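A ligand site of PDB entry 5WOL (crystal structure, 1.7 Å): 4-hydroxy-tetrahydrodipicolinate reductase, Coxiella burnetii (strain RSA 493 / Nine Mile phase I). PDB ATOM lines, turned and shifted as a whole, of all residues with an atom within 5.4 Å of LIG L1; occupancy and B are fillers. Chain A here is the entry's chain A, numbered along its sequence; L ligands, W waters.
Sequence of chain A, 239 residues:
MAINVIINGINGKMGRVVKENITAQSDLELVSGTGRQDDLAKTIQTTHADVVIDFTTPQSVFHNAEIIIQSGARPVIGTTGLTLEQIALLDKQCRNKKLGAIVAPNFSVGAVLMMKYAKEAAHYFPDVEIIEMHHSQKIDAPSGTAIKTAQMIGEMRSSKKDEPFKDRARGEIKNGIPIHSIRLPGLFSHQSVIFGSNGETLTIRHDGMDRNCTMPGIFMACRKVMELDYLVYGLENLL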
ATOM      1  N   ASN A   8       7.587  12.530   1.779  1.00  0.00           N
ATOM      2  CA  ASN A   8       6.389  12.260   1.009  1.00  0.00           C
ATOM      3  C   ASN A   8       6.653  11.068   0.103  1.00  0.00           C
ATOM      4  O   ASN A   8       7.631  11.083  -0.663  1.00  0.00           O
ATOM      5  CB  ASN A   8       6.018  13.475   0.186  1.00  0.00           C
ATOM      6  CG  ASN A   8       4.593  13.404  -0.349  1.00  0.00           C
ATOM      7  OD1 ASN A   8       3.657  12.874   0.305  1.00  0.00           O
ATOM      8  ND2 ASN A   8       4.415  13.955  -1.543  1.00  0.00           N
ATOM      9  N   GLY A   9       5.777  10.062   0.166  1.00  0.00           N
ATOM     10  CA  GLY A   9       6.056   8.767  -0.438  1.00  0.00           C
ATOM     11  C   GLY A   9       6.709   7.807   0.535  1.00  0.00           C
ATOM     12  O   GLY A   9       7.452   6.916   0.098  1.00  0.00           O
ATOM     13  N   ILE A  10       6.427   7.941   1.827  1.00  0.00           N
ATOM     14  CA  ILE A  10       7.108   7.227   2.905  1.00  0.00           C
ATOM     15  C   ILE A  10       7.061   5.722   2.752  1.00  0.00           C
ATOM     16  O   ILE A  10       7.949   5.022   3.262  1.00  0.00           O
ATOM     17  CB  ILE A  10       6.497   7.638   4.259  1.00  0.00           C
ATOM     18  CG1 ILE A  10       7.278   7.040   5.426  1.00  0.00           C
ATOM     19  CG2 ILE A  10       5.019   7.242   4.317  1.00  0.00           C
ATOM     20  CD1 ILE A  10       8.565   7.752   5.695  1.00  0.00           C
ATOM     21  N   ASN A  11       6.064   5.189   2.048  1.00  0.00           N
ATOM     22  CA  ASN A  11       5.951   3.742   1.930  1.00  0.00           C
ATOM     23  C   ASN A  11       6.668   3.195   0.705  1.00  0.00           C
ATOM     24  O   ASN A  11       6.754   1.960   0.565  1.00  0.00           O
ATOM     25  CB  ASN A  11       4.480   3.310   1.887  1.00  0.00           C
ATOM     26  CG  ASN A  11       3.744   3.594   3.185  1.00  0.00           C
ATOM     27  OD1 ASN A  11       4.348   3.630   4.254  1.00  0.00           O
ATOM     28  ND2 ASN A  11       2.432   3.805   3.095  1.00  0.00           N
ATOM     29  N   GLY A  12       7.158   4.055  -0.185  1.00  0.00           N
ATOM     30  CA  GLY A  12       7.816   3.577  -1.382  1.00  0.00           C
ATOM     31  C   GLY A  12       9.207   3.017  -1.082  1.00  0.00           C
ATOM     32  O   GLY A  12       9.731   3.122   0.020  1.00  0.00           O
ATOM     33  N   LYS A  13       9.819   2.452  -2.123  1.00  0.00           N
ATOM     34  CA  LYS A  13      11.164   1.919  -1.995  1.00  0.00           C
ATOM     35  C   LYS A  13      12.140   2.992  -1.518  1.00  0.00           C
ATOM     36  O   LYS A  13      12.863   2.792  -0.536  1.00  0.00           O
ATOM     37  CB  LYS A  13      11.611   1.296  -3.319  1.00  0.00           C
ATOM     38  CG  LYS A  13      10.739   0.131  -3.759  1.00  0.00           C
ATOM     39  CD  LYS A  13      11.443  -0.774  -4.787  1.00  0.00           C
ATOM     40  CE  LYS A  13      11.392  -0.174  -6.197  1.00  0.00           C
ATOM     41  NZ  LYS A  13      10.019   0.223  -6.652  1.00  0.00           N
ATOM     42  N   MET A  14      12.133   4.171  -2.170  1.00  0.00           N
ATOM     43  CA  MET A  14      13.039   5.235  -1.712  1.00  0.00           C
ATOM     44  C   MET A  14      12.599   5.848  -0.381  1.00  0.00           C
ATOM     45  O   MET A  14      13.444   6.124   0.473  1.00  0.00           O
ATOM     46  CB  MET A  14      13.220   6.341  -2.759  1.00  0.00           C
ATOM     47  CG  MET A  14      13.853   5.874  -4.001  1.00  0.00           C
ATOM     48  SD  MET A  14      15.632   5.765  -3.678  1.00  0.00           S
ATOM     49  CE  MET A  14      15.971   7.139  -2.562  1.00  0.00           C
ATOM     50  N   GLY A  15      11.304   6.107  -0.191  1.00  0.00           N
ATOM     51  CA  GLY A  15      10.855   6.683   1.067  1.00  0.00           C
ATOM     52  C   GLY A  15      11.252   5.833   2.255  1.00  0.00           C
ATOM     53  O   GLY A  15      11.624   6.360   3.309  1.00  0.00           O
ATOM     54  N   THR A  34       4.464  10.833   4.802  1.00  0.00           N
ATOM     55  CA  THR A  34       3.127  10.915   4.223  1.00  0.00           C
ATOM     56  C   THR A  34       3.052  10.037   2.975  1.00  0.00           C
ATOM     57  O   THR A  34       4.046   9.818   2.278  1.00  0.00           O
ATOM     58  CB  THR A  34       2.734  12.361   3.841  1.00  0.00           C
ATOM     59  OG1 THR A  34       3.791  12.937   3.068  1.00  0.00           O
ATOM     60  CG2 THR A  34       2.484  13.208   5.095  1.00  0.00           C
ATOM     61  N   GLY A  35       1.849   9.554   2.721  1.00  0.00           N
ATOM     62  CA  GLY A  35       1.618   8.701   1.584  1.00  0.00           C
ATOM     63  C   GLY A  35       0.504   9.236   0.720  1.00  0.00           C
ATOM     64  O   GLY A  35       0.032  10.367   0.915  1.00  0.00           O
ATOM     65  N   ARG A  36       0.040   8.403  -0.211  1.00  0.00           N
ATOM     66  CA  ARG A  36      -0.863   8.856  -1.264  1.00  0.00           C
ATOM     67  C   ARG A  36      -2.131   9.490  -0.709  1.00  0.00           C
ATOM     68  O   ARG A  36      -2.581  10.531  -1.205  1.00  0.00           O
ATOM     69  CB  ARG A  36      -1.194   7.683  -2.180  1.00  0.00           C
ATOM     70  CG  ARG A  36      -1.753   8.108  -3.496  1.00  0.00           C
ATOM     71  CD  ARG A  36      -2.482   6.974  -4.180  1.00  0.00           C
ATOM     72  NE  ARG A  36      -1.598   5.858  -4.482  1.00  0.00           N
ATOM     73  CZ  ARG A  36      -1.179   5.531  -5.703  1.00  0.00           C
ATOM     74  NH1 ARG A  36      -1.563   6.236  -6.776  1.00  0.00           N
ATOM     75  NH2 ARG A  36      -0.376   4.498  -5.865  1.00  0.00           N
ATOM     76  N   GLN A  37      -2.723   8.894   0.333  1.00  0.00           N
ATOM     77  CA  GLN A  37      -4.016   9.351   0.823  1.00  0.00           C
ATOM     78  C   GLN A  37      -3.924  10.270   2.031  1.00  0.00           C
ATOM     79  O   GLN A  37      -4.942  10.572   2.659  1.00  0.00           O
ATOM     80  CB  GLN A  37      -4.901   8.134   1.139  1.00  0.00           C
ATOM     81  CG  GLN A  37      -5.149   7.244  -0.078  1.00  0.00           C
ATOM     82  CD  GLN A  37      -5.130   5.768   0.272  1.00  0.00           C
ATOM     83  OE1 GLN A  37      -5.752   5.345   1.242  1.00  0.00           O
ATOM     84  NE2 GLN A  37      -4.399   4.982  -0.509  1.00  0.00           N
ATOM     85  N   PHE A  55       9.472  11.459  -3.053  1.00  0.00           N
ATOM     86  CA  PHE A  55       9.761  10.305  -3.913  1.00  0.00           C
ATOM     87  C   PHE A  55       8.425   9.613  -4.192  1.00  0.00           C
ATOM     88  O   PHE A  55       8.106   8.614  -3.539  1.00  0.00           O
ATOM     89  CB  PHE A  55      10.739   9.369  -3.266  1.00  0.00           C
ATOM     90  CG  PHE A  55      12.191   9.847  -3.365  1.00  0.00           C
ATOM     91  CD1 PHE A  55      12.905   9.709  -4.544  1.00  0.00           C
ATOM     92  CD2 PHE A  55      12.787  10.483  -2.278  1.00  0.00           C
ATOM     93  CE1 PHE A  55      14.228  10.156  -4.624  1.00  0.00           C
ATOM     94  CE2 PHE A  55      14.088  10.950  -2.351  1.00  0.00           C
ATOM     95  CZ  PHE A  55      14.829  10.770  -3.502  1.00  0.00           C
ATOM     96  N   THR A  56       7.675  10.114  -5.191  1.00  0.00           N
ATOM     97  CA  THR A  56       6.307   9.720  -5.417  1.00  0.00           C
ATOM     98  C   THR A  56       6.174   9.231  -6.865  1.00  0.00           C
ATOM     99  O   THR A  56       6.784   8.216  -7.216  1.00  0.00           O
ATOM    100  CB  THR A  56       5.312  10.832  -5.029  1.00  0.00           C
ATOM    101  OG1 THR A  56       5.459  11.989  -5.871  1.00  0.00           O
ATOM    102  CG2 THR A  56       5.516  11.242  -3.580  1.00  0.00           C
ATOM    103  N   THR A  57       5.384   9.894  -7.689  1.00  0.00           N
ATOM    104  CA  THR A  57       5.053   9.410  -9.029  1.00  0.00           C
ATOM    105  C   THR A  57       5.137  10.572 -10.002  1.00  0.00           C
ATOM    106  O   THR A  57       4.899  11.716  -9.600  1.00  0.00           O
ATOM    107  CB  THR A  57       3.618   8.829  -9.096  1.00  0.00           C
ATOM    108  OG1 THR A  57       2.681   9.867  -8.843  1.00  0.00           O
ATOM    109  CG2 THR A  57       3.429   7.733  -8.042  1.00  0.00           C
ATOM    110  N   PRO A  58       5.439  10.307 -11.278  1.00  0.00           N
ATOM    111  CA  PRO A  58       5.453  11.410 -12.258  1.00  0.00           C
ATOM    112  C   PRO A  58       4.110  12.073 -12.409  1.00  0.00           C
ATOM    113  O   PRO A  58       4.067  13.268 -12.722  1.00  0.00           O
ATOM    114  CB  PRO A  58       5.919  10.715 -13.548  1.00  0.00           C
ATOM    115  CG  PRO A  58       6.704   9.516 -13.088  1.00  0.00           C
ATOM    116  CD  PRO A  58       5.991   9.060 -11.827  1.00  0.00           C
ATOM    117  N   SER A  60       2.070  12.867 -10.010  1.00  0.00           N
ATOM    118  CA  SER A  60       1.778  13.730  -8.879  1.00  0.00           C
ATOM    119  C   SER A  60       2.859  14.771  -8.602  1.00  0.00           C
ATOM    120  O   SER A  60       2.598  15.720  -7.855  1.00  0.00           O
ATOM    121  CB  SER A  60       1.609  12.904  -7.592  1.00  0.00           C
ATOM    122  OG  SER A  60       0.435  12.122  -7.630  1.00  0.00           O
ATOM    123  N   ASN A  64       2.470  18.075  -6.288  1.00  0.00           N
ATOM    124  CA  ASN A  64       3.078  17.980  -4.961  1.00  0.00           C
ATOM    125  C   ASN A  64       4.013  19.164  -4.723  1.00  0.00           C
ATOM    126  O   ASN A  64       4.000  19.769  -3.648  1.00  0.00           O
ATOM    127  CB  ASN A  64       3.863  16.666  -4.839  1.00  0.00           C
ATOM    128  CG  ASN A  64       2.949  15.478  -4.736  1.00  0.00           C
ATOM    129  OD1 ASN A  64       1.718  15.646  -4.752  1.00  0.00           O
ATOM    130  ND2 ASN A  64       3.516  14.274  -4.630  1.00  0.00           N
ATOM    131  N   ILE A  77      13.104  17.320  -4.399  1.00  0.00           N
ATOM    132  CA  ILE A  77      12.323  16.464  -5.266  1.00  0.00           C
ATOM    133  C   ILE A  77      13.249  15.506  -5.998  1.00  0.00           C
ATOM    134  O   ILE A  77      14.086  15.962  -6.783  1.00  0.00           O
ATOM    135  CB  ILE A  77      11.524  17.296  -6.275  1.00  0.00           C
ATOM    136  CG1 ILE A  77      10.676  18.293  -5.542  1.00  0.00           C
ATOM    137  CG2 ILE A  77      10.725  16.381  -7.181  1.00  0.00           C
ATOM    138  CD1 ILE A  77       9.938  19.163  -6.496  1.00  0.00           C
ATOM    139  N   GLY A  78      13.071  14.205  -5.775  1.00  0.00           N
ATOM    140  CA  GLY A  78      13.819  13.207  -6.499  1.00  0.00           C
ATOM    141  C   GLY A  78      12.959  12.559  -7.568  1.00  0.00           C
ATOM    142  O   GLY A  78      13.474  11.981  -8.524  1.00  0.00           O
ATOM    143  N   THR A  79      11.657  12.578  -7.368  1.00  0.00           N
ATOM    144  CA  THR A  79      10.713  12.036  -8.331  1.00  0.00           C
ATOM    145  C   THR A  79      11.060  12.497  -9.750  1.00  0.00           C
ATOM    146  O   THR A  79      11.380  13.669  -9.985  1.00  0.00           O
ATOM    147  CB  THR A  79       9.302  12.509  -7.991  1.00  0.00           C
ATOM    148  OG1 THR A  79       9.063  12.329  -6.603  1.00  0.00           O
ATOM    149  CG2 THR A  79       8.291  11.700  -8.800  1.00  0.00           C
ATOM    150  N   THR A  80      10.971  11.567 -10.696  1.00  0.00           N
ATOM    151  CA  THR A  80      11.112  11.937 -12.097  1.00  0.00           C
ATOM    152  C   THR A  80       9.773  12.437 -12.644  1.00  0.00           C
ATOM    153  O   THR A  80       8.702  12.161 -12.087  1.00  0.00           O
ATOM    154  CB  THR A  80      11.596  10.741 -12.904  1.00  0.00           C
ATOM    155  OG1 THR A  80      10.624   9.693 -12.784  1.00  0.00           O
ATOM    156  CG2 THR A  80      12.919  10.249 -12.329  1.00  0.00           C
ATOM    157  N   ALA A 104      16.392  17.136  -8.364  1.00  0.00           N
ATOM    158  CA  ALA A 104      17.575  16.376  -8.795  1.00  0.00           C
ATOM    159  C   ALA A 104      17.112  15.115  -9.531  1.00  0.00           C
ATOM    160  O   ALA A 104      16.518  14.216  -8.899  1.00  0.00           O
ATOM    161  CB  ALA A 104      18.446  16.017  -7.591  1.00  0.00           C
ATOM    162  N   PRO A 105      17.331  14.991 -10.849  1.00  0.00           N
ATOM    163  CA  PRO A 105      17.028  13.719 -11.540  1.00  0.00           C
ATOM    164  C   PRO A 105      17.884  12.570 -11.072  1.00  0.00           C
ATOM    165  O   PRO A 105      17.526  11.410 -11.350  1.00  0.00           O
ATOM    166  CB  PRO A 105      17.330  14.002 -13.019  1.00  0.00           C
ATOM    167  CG  PRO A 105      17.492  15.478 -13.115  1.00  0.00           C
ATOM    168  CD  PRO A 105      17.838  16.022 -11.772  1.00  0.00           C
ATOM    169  N   ASN A 106      19.035  12.867 -10.474  1.00  0.00           N
ATOM    170  CA  ASN A 106      19.922  11.836  -9.950  1.00  0.00           C
ATOM    171  C   ASN A 106      20.520  12.364  -8.670  1.00  0.00           C
ATOM    172  O   ASN A 106      21.288  13.348  -8.706  1.00  0.00           O
ATOM    173  CB  ASN A 106      21.029  11.461 -10.952  1.00  0.00           C
ATOM    174  CG  ASN A 106      21.656  10.136 -10.585  1.00  0.00           C
ATOM    175  OD1 ASN A 106      21.791   9.805  -9.384  1.00  0.00           O
ATOM    176  ND2 ASN A 106      22.004   9.339 -11.589  1.00  0.00           N
ATOM    177  N   PHE A 107      20.178  11.735  -7.541  1.00  0.00           N
ATOM    178  CA  PHE A 107      20.618  12.181  -6.231  1.00  0.00           C
ATOM    179  C   PHE A 107      21.922  11.475  -5.808  1.00  0.00           C
ATOM    180  O   PHE A 107      22.418  11.750  -4.715  1.00  0.00           O
ATOM    181  CB  PHE A 107      19.507  11.963  -5.170  1.00  0.00           C
ATOM    182  CG  PHE A 107      18.709  13.209  -4.871  1.00  0.00           C
ATOM    183  CD1 PHE A 107      19.317  14.317  -4.295  1.00  0.00           C
ATOM    184  CD2 PHE A 107      17.343  13.247  -5.121  1.00  0.00           C
ATOM    185  CE1 PHE A 107      18.606  15.455  -4.023  1.00  0.00           C
ATOM    186  CE2 PHE A 107      16.595  14.414  -4.829  1.00  0.00           C
ATOM    187  CZ  PHE A 107      17.233  15.523  -4.279  1.00  0.00           C
ATOM    188  N   SER A 108      22.487  10.612  -6.660  1.00  0.00           N
ATOM    189  CA  SER A 108      23.792   9.981  -6.354  1.00  0.00           C
ATOM    190  C   SER A 108      24.938  10.957  -6.643  1.00  0.00           C
ATOM    191  O   SER A 108      25.161  11.347  -7.796  1.00  0.00           O
ATOM    192  CB  SER A 108      23.959   8.696  -7.192  1.00  0.00           C
ATOM    193  OG  SER A 108      25.362   8.339  -7.188  1.00  0.00           O
ATOM    194  N   ARG A 211      20.089   1.461  -2.722  1.00  0.00           N
ATOM    195  CA  ARG A 211      19.521   2.799  -2.688  1.00  0.00           C
ATOM    196  C   ARG A 211      20.171   3.728  -1.663  1.00  0.00           C
ATOM    197  O   ARG A 211      19.875   4.930  -1.687  1.00  0.00           O
ATOM    198  CB  ARG A 211      18.000   2.734  -2.406  1.00  0.00           C
ATOM    199  CG  ARG A 211      17.261   2.141  -3.578  1.00  0.00           C
ATOM    200  CD  ARG A 211      15.743   2.007  -3.341  1.00  0.00           C
ATOM    201  NE  ARG A 211      15.150   1.488  -4.572  1.00  0.00           N
ATOM    202  CZ  ARG A 211      15.129   0.201  -4.926  1.00  0.00           C
ATOM    203  NH1 ARG A 211      15.644  -0.732  -4.124  1.00  0.00           N
ATOM    204  NH2 ARG A 211      14.602  -0.161  -6.089  1.00  0.00           N
ATOM    205  N   THR A 214      21.981   7.218  -2.901  1.00  0.00           N
ATOM    206  CA  THR A 214      21.461   8.565  -3.068  1.00  0.00           C
ATOM    207  C   THR A 214      21.398   9.351  -1.769  1.00  0.00           C
ATOM    208  O   THR A 214      21.082  10.542  -1.803  1.00  0.00           O
ATOM    209  CB  THR A 214      20.061   8.527  -3.664  1.00  0.00           C
ATOM    210  OG1 THR A 214      19.253   7.757  -2.784  1.00  0.00           O
ATOM    211  CG2 THR A 214      20.078   7.885  -5.038  1.00  0.00           C
HETATM  212  P1  LIG L   1       7.780   3.433  -5.540  1.00  0.00           P
HETATM  213  O1  LIG L   1       8.395   2.245  -4.863  1.00  0.00           O
HETATM  214  O2  LIG L   1       6.678   3.100  -6.476  1.00  0.00           O
HETATM  215  O3  LIG L   1       7.248   4.466  -4.431  1.00  0.00           O
HETATM  216  C1  LIG L   1       6.440   5.578  -4.755  1.00  0.00           C
HETATM  217  C2  LIG L   1       5.657   5.933  -3.492  1.00  0.00           C
HETATM  218  O4  LIG L   1       4.918   7.130  -3.673  1.00  0.00           O
HETATM  219  C3  LIG L   1       4.641   4.854  -3.122  1.00  0.00           C
HETATM  220  O5  LIG L   1       4.765   4.556  -1.750  1.00  0.00           O
HETATM  221  C4  LIG L   1       3.269   5.473  -3.383  1.00  0.00           C
HETATM  222  O6  LIG L   1       2.267   5.061  -2.465  1.00  0.00           O
HETATM  223  C5  LIG L   1       3.595   6.935  -3.157  1.00  0.00           C
HETATM  224  N1  LIG L   1       2.654   7.852  -3.825  1.00  0.00           N
HETATM  225  C6  LIG L   1       2.016   7.731  -5.027  1.00  0.00           C
HETATM  226  N2  LIG L   1       1.286   8.860  -5.246  1.00  0.00           N
HETATM  227  C7  LIG L   1       1.453   9.707  -4.199  1.00  0.00           C
HETATM  228  C8  LIG L   1       0.959  10.984  -3.900  1.00  0.00           C
HETATM  229  N3  LIG L   1       0.104  11.646  -4.693  1.00  0.00           N
HETATM  230  N4  LIG L   1       1.357  11.575  -2.707  1.00  0.00           N
HETATM  231  C9  LIG L   1       2.215  10.929  -1.835  1.00  0.00           C
HETATM  232  N5  LIG L   1       2.709   9.663  -2.148  1.00  0.00           N
HETATM  233  C10 LIG L   1       2.330   9.070  -3.304  1.00  0.00           C
HETATM  234  O7  LIG L   1       8.882   4.252  -6.370  1.00  0.00           O
HETATM  235  P2  LIG L   1      10.395   4.609  -5.980  1.00  0.00           P
HETATM  236  O8  LIG L   1      11.291   3.521  -6.479  1.00  0.00           O
HETATM  237  O9  LIG L   1      10.423   4.979  -4.551  1.00  0.00           O
HETATM  238  O10 LIG L   1      10.630   5.958  -6.865  1.00  0.00           O
HETATM  239  C11 LIG L   1       9.927   7.187  -6.624  1.00  0.00           C
HETATM  240  C12 LIG L   1      10.197   8.206  -7.726  1.00  0.00           C
HETATM  241  O11 LIG L   1      11.518   8.712  -7.549  1.00  0.00           O
HETATM  242  C13 LIG L   1      10.160   7.605  -9.130  1.00  0.00           C
HETATM  243  O12 LIG L   1       9.739   8.584 -10.066  1.00  0.00           O
HETATM  244  C14 LIG L   1      11.616   7.239  -9.399  1.00  0.00           C
HETATM  245  O13 LIG L   1      11.966   7.238 -10.760  1.00  0.00           O
HETATM  246  C15 LIG L   1      12.307   8.381  -8.682  1.00  0.00           C
HETATM  247  N6  LIG L   1      13.666   8.075  -8.224  1.00  0.00           N
HETATM  248  C16 LIG L   1      14.547   9.074  -8.359  1.00  0.00           C
HETATM  249  C17 LIG L   1      15.844   8.879  -7.936  1.00  0.00           C
HETATM  250  C18 LIG L   1      16.687  10.101  -7.921  1.00  0.00           C
HETATM  251  O14 LIG L   1      18.014   9.871  -7.618  1.00  0.00           O
HETATM  252  N7  LIG L   1      16.140  11.303  -8.218  1.00  0.00           N
HETATM  253  C19 LIG L   1      16.274   7.684  -7.349  1.00  0.00           C
HETATM  254  C20 LIG L   1      15.342   6.674  -7.197  1.00  0.00           C
HETATM  255  C21 LIG L   1      14.031   6.890  -7.634  1.00  0.00           C
HETATM  256  P3  LIG L   1       1.520   3.625  -2.638  1.00  0.00           P
HETATM  257  O15 LIG L   1       0.185   3.763  -1.938  1.00  0.00           O
HETATM  258  O16 LIG L   1       1.309   3.276  -4.092  1.00  0.00           O
HETATM  259  O17 LIG L   1       2.370   2.548  -1.977  1.00  0.00           O
HETATM  260  C1  LG2 L   2      17.719   3.081  -8.473  1.00  0.00           C
HETATM  261  C2  LG2 L   2      19.780   4.210  -8.561  1.00  0.00           C
HETATM  262  C3  LG2 L   2      19.550   4.737  -7.298  1.00  0.00           C
HETATM  263  C4  LG2 L   2      16.684   2.155  -9.118  1.00  0.00           C
HETATM  264  C5  LG2 L   2      18.408   4.425  -6.626  1.00  0.00           C
HETATM  265  C6  LG2 L   2      17.496   3.607  -7.202  1.00  0.00           C
HETATM  266  O1  LG2 L   2      15.704   1.753  -8.433  1.00  0.00           O
HETATM  267  O2  LG2 L   2      16.803   1.805 -10.317  1.00  0.00           O
HETATM  268  N1  LG2 L   2      18.868   3.392  -9.137  1.00  0.00           N
HETATM  269  O   HOH W   1       1.231   5.566   0.199  1.00  0.00           O
HETATM  270  O   HOH W   2       7.535   2.753  -9.109  1.00  0.00           O
HETATM  271  O   HOH W   3       9.311   6.264  -2.349  1.00  0.00           O
HETATM  272  O   HOH W   4       3.955   6.275   0.164  1.00  0.00           O
HETATM  273  O   HOH W   5       0.038   9.468  -7.854  1.00  0.00           O
HETATM  274  O   HOH W   6       8.670   6.840 -11.954  1.00  0.00           O
HETATM  275  O   HOH W   7       6.655   5.843  -8.623  1.00  0.00           O
HETATM  276  O   HOH W   8       1.373  14.230  -2.054  1.00  0.00           O
HETATM  277  O   HOH W   9      13.813   3.287  -6.241  1.00  0.00           O
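OD1 of Asn 8 touches C9 of LIG L1 (3.2 Å).
Gly 9 touches LIG L1.
Asn 11 touches LIG L1 (C to O5, 3.4 Å).
Gly 35 touches LIG L1 (C to C9, 3.5 Å).
CD1 of Phe 55 touches O11 of LIG L1, 3.5 Å away.
O of Thr 56 touches C11 of LIG L1, at 3.4 Å.
CG2 of Thr 57 touches C6 of LIG L1, at 3.3 Å.
Asn 64 touches LIG L1 (ND2 to N4, 3.96 Å).
Thr 79 touches LIG L1 (CA to O11, 3.5 Å).
CA of Asn 106 touches O14 of LIG L1 (3.6 Å).
Thr 214 touches LIG L1 (CG2 to O14, 3.9 Å).
Hydrophobic or aromatic side chains within 4 Å of LIG L1: Met 14, Phe 55 and Phe 107.
Within 4 Å of LIG L1: Asn 8, Gly 9, Asn 11, Gly 12, Lys 13, Met 14, Gly 35, Arg 36, Phe 55, Thr 56, Thr 57, Ser 60, Asn 64, Gly 78, Thr 79, Thr 80, Ala 104, Pro 105, Asn 106, Phe 107 and Thr 214.
NH2 of Arg 36 is in salt-bridge range of O16 of LIG L1 (2.7 Å).
O of Gly 78 sits at hydrogen-bond distance from N7 of LIG L1.
The backbone NH (N) of Phe 107 sits at hydrogen-bond distance from an oxygen (O14) of LIG L1, at 2.9 Å.
The backbone NH (N) of Gly 12 sits at hydrogen-bond distance from an oxygen (O5) of LIG L1.
OG of Ser 60 lies within hydrogen-bond range of N3 of LIG L1, at 3.0 Å.
The backbone carbonyl oxygen of Ala 104 lies within hydrogen-bond range of a nitrogen (N7) of LIG L1.
The backbone NH of Met 14 is in hydrogen-bond range of an oxygen (O9) of LIG L1 (3.0 Å).
The backbone NH (N) of Thr 80 lies within hydrogen-bond range of an oxygen (O12) of LIG L1 (3.3 Å).
OG1 of Thr 80 is in hydrogen-bond range of O12 of LIG L1.
The backbone NH of Lys 13 sits at hydrogen-bond distance from an oxygen (O1) of LIG L1.
The side-chain amino group of Lys 13 lies within salt-bridge range of an oxygen (O1) of LIG L1, at 3.2 Å.
The backbone carbonyl oxygen (O) of Pro 105 lies within hydrogen-bond range of a nitrogen (N7) of LIG L1 (3.4 Å).
O1 of LG2 L2 lies within salt-bridge range of NH2 of Arg 211 (3.2 Å).
The backbone carbonyl oxygen of Ile 77 sits at hydrogen-bond distance from the backbone NH of Ala 104.
The backbone carbonyl oxygen of Asn 8 is in hydrogen-bond range of the backbone NH of Phe 55 (3.0 Å).
The side-chain amide nitrogen of Asn 8 sits close to the side-chain amide nitrogen of Asn 64 (3.2 Å).
The side-chain amide oxygen (OD1) of Asn 8 lies within hydrogen-bond range of the side-chain hydroxyl (OG1) of Thr 34 (2.8 Å).
The side-chain hydroxyl of Thr 79 is in hydrogen-bond range of the backbone NH of Thr 56.
OG1 of Thr 56 sits at hydrogen-bond distance from ND2 of Asn 64, 3.2 Å away.
OD1 of Asn 106 lies within hydrogen-bond range of N of Ser 108 (2.9 Å).
The backbone NH (N) of Gly 9 is in hydrogen-bond range of the backbone carbonyl oxygen (O) of Thr 34.
Water W9 lies within hydrogen-bond range of an oxygen (O8) of LIG L1 (2.5 Å), the guanidinium group (NE) of Arg 211 (2.8 Å) and an oxygen (O1) of LG2 L2 (3.3 Å).
Water W4 lies within hydrogen-bond range of an oxygen (O5) of LIG L1, the backbone NH of Asn 11 and the backbone NH of Ile 10.
Water W8 lies within hydrogen-bond range of N4 of LIG L1 (2.7 Å), OD1 of Asn 64 (3.1 Å) and ND2 of Asn 8 (3.1 Å).
Water W3 lies within hydrogen-bond range of an oxygen (O9) of LIG L1 (2.8 Å), the backbone carbonyl oxygen (O) of Phe 55 (2.9 Å), the backbone NH (N) of Gly 15 (2.9 Å) and the backbone carbonyl oxygen (O) of Gly 9 (3.1 Å).
Water W5 lies within hydrogen-bond range of the side-chain hydroxyl (OG) of Ser 60 (2.7 Å), the side-chain hydroxyl (OG1) of Thr 57 (2.9 Å) and a nitrogen (N2) of LIG L1 (3.0 Å).
Water W7 lies within hydrogen-bond range of the backbone carbonyl oxygen (O) of Thr 56 (2.8 Å) and an oxygen (O2) of LIG L1 (3.5 Å).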
